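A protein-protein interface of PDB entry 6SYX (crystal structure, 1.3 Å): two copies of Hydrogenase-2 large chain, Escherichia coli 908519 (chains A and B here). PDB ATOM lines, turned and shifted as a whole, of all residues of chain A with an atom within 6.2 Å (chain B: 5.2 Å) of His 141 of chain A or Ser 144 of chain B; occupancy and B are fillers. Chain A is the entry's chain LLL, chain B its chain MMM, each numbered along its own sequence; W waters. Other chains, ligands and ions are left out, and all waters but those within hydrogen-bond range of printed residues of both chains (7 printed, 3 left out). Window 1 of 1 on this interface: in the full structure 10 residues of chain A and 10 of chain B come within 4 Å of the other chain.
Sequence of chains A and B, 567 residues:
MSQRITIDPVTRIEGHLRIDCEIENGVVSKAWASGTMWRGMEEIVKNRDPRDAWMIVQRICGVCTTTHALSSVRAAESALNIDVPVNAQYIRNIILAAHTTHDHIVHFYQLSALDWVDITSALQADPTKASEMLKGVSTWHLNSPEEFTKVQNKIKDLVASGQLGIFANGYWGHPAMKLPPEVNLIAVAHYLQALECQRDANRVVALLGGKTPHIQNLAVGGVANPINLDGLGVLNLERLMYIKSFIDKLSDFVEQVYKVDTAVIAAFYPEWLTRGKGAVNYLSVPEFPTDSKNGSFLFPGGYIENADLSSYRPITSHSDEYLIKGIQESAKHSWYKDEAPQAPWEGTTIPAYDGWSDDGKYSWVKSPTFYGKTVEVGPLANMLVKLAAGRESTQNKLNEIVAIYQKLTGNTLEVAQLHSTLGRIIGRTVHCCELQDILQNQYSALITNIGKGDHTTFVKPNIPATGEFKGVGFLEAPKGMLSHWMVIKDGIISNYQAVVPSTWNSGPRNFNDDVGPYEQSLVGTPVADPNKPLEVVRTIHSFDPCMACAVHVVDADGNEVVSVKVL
Lys 135 of chain A touches Pro 145 of chain B (NZ to CG, 3.7 Å). Glu 146 of chain B touches Thr 139 of chain A (CB to O, 3.6 Å). O of Trp 140 of chain A touches CB of Glu 146 of chain B (3.5 Å). ND1 of His 141 of chain A touches CD2 of Leu 142 of chain B, at 3.6 Å. ND1 of His 141 of chain A touches CE of Lys 150 of chain B, at 3.9 Å. Leu 142 of chain A touches His 141 of chain B. CD2 of Leu 142 of chain A touches CD2 of Leu 142 of chain B, 3.6 Å away.
NZ of Lys 150 of chain B lies within salt-bridge range of OE1 of Glu 147 of chain B. OG of Ser 144 of chain B lies within hydrogen-bond range of N of Glu 147 of chain B (3.0 Å). The side-chain hydroxyl (OG) of Ser 138 of chain A lies within hydrogen-bond range of the backbone NH (N) of Trp 140 of chain A, 2.9 Å away. The backbone carbonyl oxygen of Pro 145 of chain B sits at hydrogen-bond distance from the side-chain hydroxyl of Thr 149 of chain B. OG of Ser 144 of chain A sits close to N of Glu 146 of chain A.
Of the printed residues of chain B, Lys 135 of chain A touches Pro 145 (3.7 Å) and Glu 146 (2.9 Å). Of chain B, only Leu 142, Ser 144, Glu 147 and Lys 150 come within 4 Å of His 141 of chain A. Of the printed residues of chain B, Leu 142 of chain A touches His 141 and Leu 142. Asn 143 of chain A touches none of the printed residues of chain B. Printed residues of chain A within 4 Å of His 141 of chain B: Leu 142 (3.6 Å) and Ser 144 (3.3 Å). Of the printed residues of chain A, Leu 142 of chain B touches His 141 (3.6 Å) and Leu 142 (3.6 Å). Of chain A, only His 141 (3.3 Å) comes within 4 Å of Ser 144 of chain B. Printed residues of chain A within 4 Å of Glu 147 of chain B: His 141.
Hydrophobic or aromatic side chains of chain A within 4 Å of the printed part of chain B: His 141 and Leu 142. Along chain A the printed residues that touch a printed residue of chain B span positions 135 to 144. Of the 11 printed residues of chain B, 7 touch a printed residue of chain A. Hydrophobic or aromatic side chains of chain B within 4 Å of the printed part of chain A: His 141, Leu 142 and Pro 145. Along chain B the printed residues that touch a printed residue of chain A span positions 141 to 150. Among the printed residues, 11 pairs touch across the chains. Among the printed residues, Asp or Glu carboxylates within 4 Å of a Lys or Arg side-chain nitrogen of the other chain: Lys 135 of chain A with Glu 146 of chain B.
OG of Ser 144 of chain B lies within hydrogen-bond range of O of His 141 of chain A (3.3 Å). O of His 141 of chain B is in hydrogen-bond range of OG of Ser 144 of chain A (3.3 Å). The side-chain amino group of Lys 135 of chain A lies within salt-bridge range of the side-chain carboxylate of Glu 146 of chain B (2.9 Å). The side-chain carboxylate (OE1) of Glu 147 of chain B is in hydrogen-bond range of a ring nitrogen (ND1) of His 141 of chain A (2.8 Å).
His 141 of chain A touches Leu 142 of chain B, and with the chains exchanged Leu 142 of chain A touches His 141 of chain B. His 141 of chain A touches Ser 144 of chain B, and with the chains exchanged Ser 144 of chain A touches His 141 of chain B. Leu 142 of chain A touches its own counterpart, Leu 142 of chain B. Positions printed for both chains: 141, 142, 143, 144 and 146.
Water W5 bridges OE1 of Glu 146 of chain B (2.7 Å) and O of Asn 143 of chain A (3.3 Å). Water W1 bridges the backbone carbonyl oxygen (O) of Ser 138 of chain A (2.7 Å) and the side-chain carboxylate (OE2) of Glu 146 of chain B (2.9 Å). Water W4 lies within hydrogen-bond range of OE2 of Glu 147 of chain B and ND1 of His 141 of chain A. Water W6 bridges OE2 of Glu 146 of chain B and O of Ser 138 of chain A. Water W2 bridges O of Glu 146 of chain B (2.9 Å) and O of Thr 139 of chain A (3.4 Å). Water W3 lies within hydrogen-bond range of N of Asn 143 of chain B (2.9 Å), OG of Ser 144 of chain A (3.0 Å), O of His 141 of chain B (3.3 Å), OE1 of Glu 146 of chain A (3.5 Å) and N of Leu 142 of chain B (3.5 Å).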
ATOM      1  N   LYS A 135      31.919  10.449  18.075  1.00  0.00           N
ATOM      2  CA  LYS A 135      31.843  10.034  19.521  1.00  0.00           C
ATOM      3  C   LYS A 135      32.928  10.724  20.336  1.00  0.00           C
ATOM      4  O   LYS A 135      34.091  10.571  19.947  1.00  0.00           O
ATOM      5  CB  LYS A 135      32.054   8.528  19.673  1.00  0.00           C
ATOM      6  CG  LYS A 135      30.996   7.715  18.994  1.00  0.00           C
ATOM      7  CD  LYS A 135      29.646   7.951  19.613  1.00  0.00           C
ATOM      8  CE  LYS A 135      28.516   7.545  18.700  1.00  0.00           C
ATOM      9  NZ  LYS A 135      27.231   7.904  19.324  1.00  0.00           N
ATOM     10  N   SER A 138      31.355  15.613  19.734  1.00  0.00           N
ATOM     11  CA  SER A 138      30.103  16.413  19.835  1.00  0.00           C
ATOM     12  C   SER A 138      29.058  15.668  20.660  1.00  0.00           C
ATOM     13  O   SER A 138      29.053  14.366  20.590  1.00  0.00           O
ATOM     14  CB  SER A 138      29.530  16.679  18.433  1.00  0.00           C
ATOM     15  OG  SER A 138      28.293  17.363  18.514  1.00  0.00           O
ATOM     16  N   THR A 139      28.191  16.405  21.321  1.00  0.00           N
ATOM     17  CA  THR A 139      26.988  15.870  22.009  1.00  0.00           C
ATOM     18  C   THR A 139      25.703  16.148  21.173  1.00  0.00           C
ATOM     19  O   THR A 139      24.585  15.906  21.694  1.00  0.00           O
ATOM     20  CB  THR A 139      26.835  16.451  23.423  1.00  0.00           C
ATOM     21  OG1 THR A 139      26.602  17.856  23.369  1.00  0.00           O
ATOM     22  CG2 THR A 139      28.019  16.169  24.346  1.00  0.00           C
ATOM     23  N   TRP A 140      25.823  16.623  19.918  1.00  0.00           N
ATOM     24  CA  TRP A 140      24.629  16.929  19.073  1.00  0.00           C
ATOM     25  C   TRP A 140      23.749  15.679  18.944  1.00  0.00           C
ATOM     26  O   TRP A 140      24.281  14.594  18.679  1.00  0.00           O
ATOM     27  CB  TRP A 140      25.083  17.448  17.721  1.00  0.00           C
ATOM     28  CG  TRP A 140      24.022  17.764  16.708  1.00  0.00           C
ATOM     29  CD1 TRP A 140      23.976  17.290  15.421  1.00  0.00           C
ATOM     30  CD2 TRP A 140      22.961  18.748  16.804  1.00  0.00           C
ATOM     31  NE1 TRP A 140      22.965  17.905  14.709  1.00  0.00           N
ATOM     32  CE2 TRP A 140      22.321  18.792  15.525  1.00  0.00           C
ATOM     33  CE3 TRP A 140      22.497  19.630  17.804  1.00  0.00           C
ATOM     34  CZ2 TRP A 140      21.262  19.666  15.254  1.00  0.00           C
ATOM     35  CZ3 TRP A 140      21.434  20.469  17.543  1.00  0.00           C
ATOM     36  CH2 TRP A 140      20.820  20.484  16.274  1.00  0.00           C
ATOM     37  N   HIS A 141      22.436  15.873  18.997  1.00  0.00           N
ATOM     38  CA  HIS A 141      21.432  14.777  18.981  1.00  0.00           C
ATOM     39  C   HIS A 141      21.122  14.251  17.570  1.00  0.00           C
ATOM     40  O   HIS A 141      20.364  13.253  17.472  1.00  0.00           O
ATOM     41  CB  HIS A 141      20.163  15.196  19.753  1.00  0.00           C
ATOM     42  CG  HIS A 141      19.264  16.195  19.102  1.00  0.00           C
ATOM     43  ND1 HIS A 141      17.914  16.281  19.410  1.00  0.00           N
ATOM     44  CD2 HIS A 141      19.496  17.184  18.209  1.00  0.00           C
ATOM     45  CE1 HIS A 141      17.368  17.271  18.709  1.00  0.00           C
ATOM     46  NE2 HIS A 141      18.320  17.830  17.939  1.00  0.00           N
ATOM     47  N   LEU A 142      21.591  14.882  16.466  1.00  0.00           N
ATOM     48  CA  LEU A 142      21.247  14.500  15.072  1.00  0.00           C
ATOM     49  C   LEU A 142      22.490  14.124  14.230  1.00  0.00           C
ATOM     50  O   LEU A 142      22.601  14.467  13.021  1.00  0.00           O
ATOM     51  CB  LEU A 142      20.426  15.627  14.433  1.00  0.00           C
ATOM     52  CG  LEU A 142      18.932  15.609  14.748  1.00  0.00           C
ATOM     53  CD1 LEU A 142      18.299  16.929  14.348  1.00  0.00           C
ATOM     54  CD2 LEU A 142      18.172  14.457  14.080  1.00  0.00           C
ATOM     55  N   ASN A 143      23.351  13.318  14.855  1.00  0.00           N
ATOM     56  CA  ASN A 143      24.547  12.707  14.219  1.00  0.00           C
ATOM     57  C   ASN A 143      24.440  11.163  14.136  1.00  0.00           C
ATOM     58  O   ASN A 143      25.500  10.494  13.925  1.00  0.00           O
ATOM     59  CB  ASN A 143      25.850  13.104  14.937  1.00  0.00           C
ATOM     60  CG  ASN A 143      26.318  14.541  14.687  1.00  0.00           C
ATOM     61  OD1 ASN A 143      26.943  15.164  15.593  1.00  0.00           O
ATOM     62  ND2 ASN A 143      26.043  15.046  13.510  1.00  0.00           N
ATOM     63  N   SER A 144      23.243  10.582  14.134  1.00  0.00           N
ATOM     64  CA  SER A 144      23.076   9.109  14.086  1.00  0.00           C
ATOM     65  C   SER A 144      23.386   8.569  12.682  1.00  0.00           C
ATOM     66  O   SER A 144      23.257   9.261  11.645  1.00  0.00           O
ATOM     67  CB  SER A 144      21.678   8.686  14.518  1.00  0.00           C
ATOM     68  OG  SER A 144      20.742   9.151  13.554  1.00  0.00           O
ATOM     69  N   GLU A 146      21.347   6.718  11.145  1.00  0.00           N
ATOM     70  CA  GLU A 146      20.023   6.774  10.480  1.00  0.00           C
ATOM     71  C   GLU A 146      19.793   8.181   9.858  1.00  0.00           C
ATOM     72  O   GLU A 146      19.349   8.274   8.704  1.00  0.00           O
ATOM     73  CB  GLU A 146      18.899   6.401  11.470  1.00  0.00           C
ATOM     74  CG  GLU A 146      18.939   4.935  11.989  1.00  0.00           C
ATOM     75  CD  GLU A 146      20.038   4.495  12.941  1.00  0.00           C
ATOM     76  OE1 GLU A 146      20.716   5.373  13.562  1.00  0.00           O
ATOM     77  OE2 GLU A 146      20.211   3.233  13.119  1.00  0.00           O
ATOM     78  N   GLN A 256      27.244  22.789  19.277  1.00  0.00           N
ATOM     79  CA  GLN A 256      27.513  21.330  19.116  1.00  0.00           C
ATOM     80  C   GLN A 256      27.703  20.953  17.646  1.00  0.00           C
ATOM     81  O   GLN A 256      28.134  19.795  17.352  1.00  0.00           O
ATOM     82  CB  GLN A 256      26.381  20.499  19.753  1.00  0.00           C
ATOM     83  CG  GLN A 256      26.063  20.813  21.220  1.00  0.00           C
ATOM     84  CD  GLN A 256      24.729  20.264  21.717  1.00  0.00           C
ATOM     85  OE1 GLN A 256      23.937  19.578  21.023  1.00  0.00           O
ATOM     86  NE2 GLN A 256      24.400  20.589  22.967  1.00  0.00           N
ATOM     87  N   SER B 131      20.501   2.666  22.401  1.00  0.00           N
ATOM     88  CA  SER B 131      20.559   2.954  20.950  1.00  0.00           C
ATOM     89  C   SER B 131      20.895   1.701  20.127  1.00  0.00           C
ATOM     90  O   SER B 131      20.252   1.415  19.112  1.00  0.00           O
ATOM     91  CB  SER B 131      21.537   4.097  20.692  1.00  0.00           C
ATOM     92  OG  SER B 131      21.543   4.442  19.321  1.00  0.00           O
ATOM     93  N   HIS B 141      15.420   8.807  12.940  1.00  0.00           N
ATOM     94  CA  HIS B 141      16.669   9.632  13.021  1.00  0.00           C
ATOM     95  C   HIS B 141      16.965  10.178  14.433  1.00  0.00           C
ATOM     96  O   HIS B 141      18.076  10.797  14.552  1.00  0.00           O
ATOM     97  CB  HIS B 141      16.585  10.741  11.974  1.00  0.00           C
ATOM     98  CG  HIS B 141      15.651  11.860  12.285  1.00  0.00           C
ATOM     99  ND1 HIS B 141      15.835  13.146  11.715  1.00  0.00           N
ATOM    100  CD2 HIS B 141      14.513  11.954  13.015  1.00  0.00           C
ATOM    101  CE1 HIS B 141      14.838  13.921  12.132  1.00  0.00           C
ATOM    102  NE2 HIS B 141      14.017  13.221  12.905  1.00  0.00           N
ATOM    103  N   LEU B 142      16.127   9.985  15.462  1.00  0.00           N
ATOM    104  CA  LEU B 142      16.331  10.528  16.837  1.00  0.00           C
ATOM    105  C   LEU B 142      16.380   9.406  17.914  1.00  0.00           C
ATOM    106  O   LEU B 142      15.836   9.557  19.035  1.00  0.00           O
ATOM    107  CB  LEU B 142      15.256  11.583  17.124  1.00  0.00           C
ATOM    108  CG  LEU B 142      15.541  12.978  16.564  1.00  0.00           C
ATOM    109  CD1 LEU B 142      14.279  13.874  16.605  1.00  0.00           C
ATOM    110  CD2 LEU B 142      16.728  13.606  17.287  1.00  0.00           C
ATOM    111  N   ASN B 143      17.141   8.352  17.585  1.00  0.00           N
ATOM    112  CA  ASN B 143      17.438   7.214  18.496  1.00  0.00           C
ATOM    113  C   ASN B 143      18.927   7.161  18.873  1.00  0.00           C
ATOM    114  O   ASN B 143      19.382   6.099  19.345  1.00  0.00           O
ATOM    115  CB  ASN B 143      16.958   5.875  17.945  1.00  0.00           C
ATOM    116  CG  ASN B 143      15.448   5.651  18.042  1.00  0.00           C
ATOM    117  OD1 ASN B 143      14.820   6.155  18.992  1.00  0.00           O
ATOM    118  ND2 ASN B 143      14.900   4.887  17.094  1.00  0.00           N
ATOM    119  N   SER B 144      19.669   8.263  18.784  1.00  0.00           N
ATOM    120  CA  SER B 144      21.119   8.282  19.097  1.00  0.00           C
ATOM    121  C   SER B 144      21.381   8.158  20.594  1.00  0.00           C
ATOM    122  O   SER B 144      20.584   8.580  21.437  1.00  0.00           O
ATOM    123  CB  SER B 144      21.792   9.532  18.544  1.00  0.00           C
ATOM    124  OG  SER B 144      21.360  10.656  19.222  1.00  0.00           O
ATOM    125  N   PRO B 145      22.601   7.690  20.978  1.00  0.00           N
ATOM    126  CA  PRO B 145      22.974   7.774  22.388  1.00  0.00           C
ATOM    127  C   PRO B 145      22.952   9.199  22.958  1.00  0.00           C
ATOM    128  O   PRO B 145      22.657   9.412  24.083  1.00  0.00           O
ATOM    129  CB  PRO B 145      24.404   7.131  22.409  1.00  0.00           C
ATOM    130  CG  PRO B 145      24.498   6.295  21.176  1.00  0.00           C
ATOM    131  CD  PRO B 145      23.609   6.992  20.162  1.00  0.00           C
ATOM    132  N   GLU B 146      23.285  10.163  22.107  1.00  0.00           N
ATOM    133  CA  GLU B 146      23.282  11.605  22.475  1.00  0.00           C
ATOM    134  C   GLU B 146      21.867  12.084  22.814  1.00  0.00           C
ATOM    135  O   GLU B 146      21.685  12.791  23.837  1.00  0.00           O
ATOM    136  CB  GLU B 146      23.979  12.400  21.375  1.00  0.00           C
ATOM    137  CG  GLU B 146      25.488  12.102  21.281  1.00  0.00           C
ATOM    138  CD  GLU B 146      25.903  10.823  20.584  1.00  0.00           C
ATOM    139  OE1 GLU B 146      25.086  10.217  19.864  1.00  0.00           O
ATOM    140  OE2 GLU B 146      27.126  10.429  20.719  1.00  0.00           O
ATOM    141  N   GLU B 147      20.876  11.715  21.973  1.00  0.00           N
ATOM    142  CA  GLU B 147      19.454  12.040  22.293  1.00  0.00           C
ATOM    143  C   GLU B 147      19.068  11.410  23.629  1.00  0.00           C
ATOM    144  O   GLU B 147      18.489  12.071  24.471  1.00  0.00           O
ATOM    145  CB  GLU B 147      18.563  11.572  21.143  1.00  0.00           C
ATOM    146  CG  GLU B 147      17.074  11.775  21.429  1.00  0.00           C
ATOM    147  CD  GLU B 147      16.546  13.195  21.371  1.00  0.00           C
ATOM    148  OE1 GLU B 147      17.375  14.176  21.216  1.00  0.00           O
ATOM    149  OE2 GLU B 147      15.282  13.387  21.394  1.00  0.00           O
ATOM    150  N   PHE B 148      19.401  10.111  23.811  1.00  0.00           N
ATOM    151  CA  PHE B 148      18.958   9.390  25.018  1.00  0.00           C
ATOM    152  C   PHE B 148      19.662   9.936  26.277  1.00  0.00           C
ATOM    153  O   PHE B 148      19.065   9.951  27.365  1.00  0.00           O
ATOM    154  CB  PHE B 148      19.137   7.878  24.855  1.00  0.00           C
ATOM    155  CG  PHE B 148      18.326   7.210  23.771  1.00  0.00           C
ATOM    156  CD1 PHE B 148      17.191   7.807  23.223  1.00  0.00           C
ATOM    157  CD2 PHE B 148      18.666   5.959  23.283  1.00  0.00           C
ATOM    158  CE1 PHE B 148      16.408   7.146  22.290  1.00  0.00           C
ATOM    159  CE2 PHE B 148      17.882   5.301  22.354  1.00  0.00           C
ATOM    160  CZ  PHE B 148      16.748   5.899  21.843  1.00  0.00           C
ATOM    161  N   THR B 149      20.911  10.400  26.145  1.00  0.00           N
ATOM    162  CA  THR B 149      21.658  11.015  27.286  1.00  0.00           C
ATOM    163  C   THR B 149      21.005  12.342  27.685  1.00  0.00           C
ATOM    164  O   THR B 149      20.799  12.585  28.873  1.00  0.00           O
ATOM    165  CB  THR B 149      23.150  11.198  26.927  1.00  0.00           C
ATOM    166  OG1 THR B 149      23.740   9.917  26.637  1.00  0.00           O
ATOM    167  CG2 THR B 149      23.880  11.904  28.051  1.00  0.00           C
ATOM    168  N   LYS B 150      20.625  13.171  26.701  1.00  0.00           N
ATOM    169  CA  LYS B 150      19.921  14.443  26.994  1.00  0.00           C
ATOM    170  C   LYS B 150      18.618  14.156  27.771  1.00  0.00           C
ATOM    171  O   LYS B 150      18.264  14.875  28.759  1.00  0.00           O
ATOM    172  CB  LYS B 150      19.715  15.182  25.657  1.00  0.00           C
ATOM    173  CG  LYS B 150      18.935  16.490  25.703  1.00  0.00           C
ATOM    174  CD  LYS B 150      18.764  17.166  24.341  1.00  0.00           C
ATOM    175  CE  LYS B 150      18.100  16.302  23.276  1.00  0.00           C
ATOM    176  NZ  LYS B 150      16.631  16.342  23.345  1.00  0.00           N
HETATM  177  O   HOH W   1      29.288  12.011  21.877  1.00  0.00           O
HETATM  178  O   HOH W   2      23.868  14.438  24.649  1.00  0.00           O
HETATM  179  O   HOH W   3      18.680   7.654  15.188  1.00  0.00           O
HETATM  180  O   HOH W   4      14.739  15.762  20.156  1.00  0.00           O
HETATM  181  O   HOH W   5      25.194   9.964  17.191  1.00  0.00           O
HETATM  182  O   HOH W   6      28.761  11.852  18.987  1.00  0.00           O
HETATM  183  O   HOH W   7      20.476   5.687  16.219  1.00  0.00           O
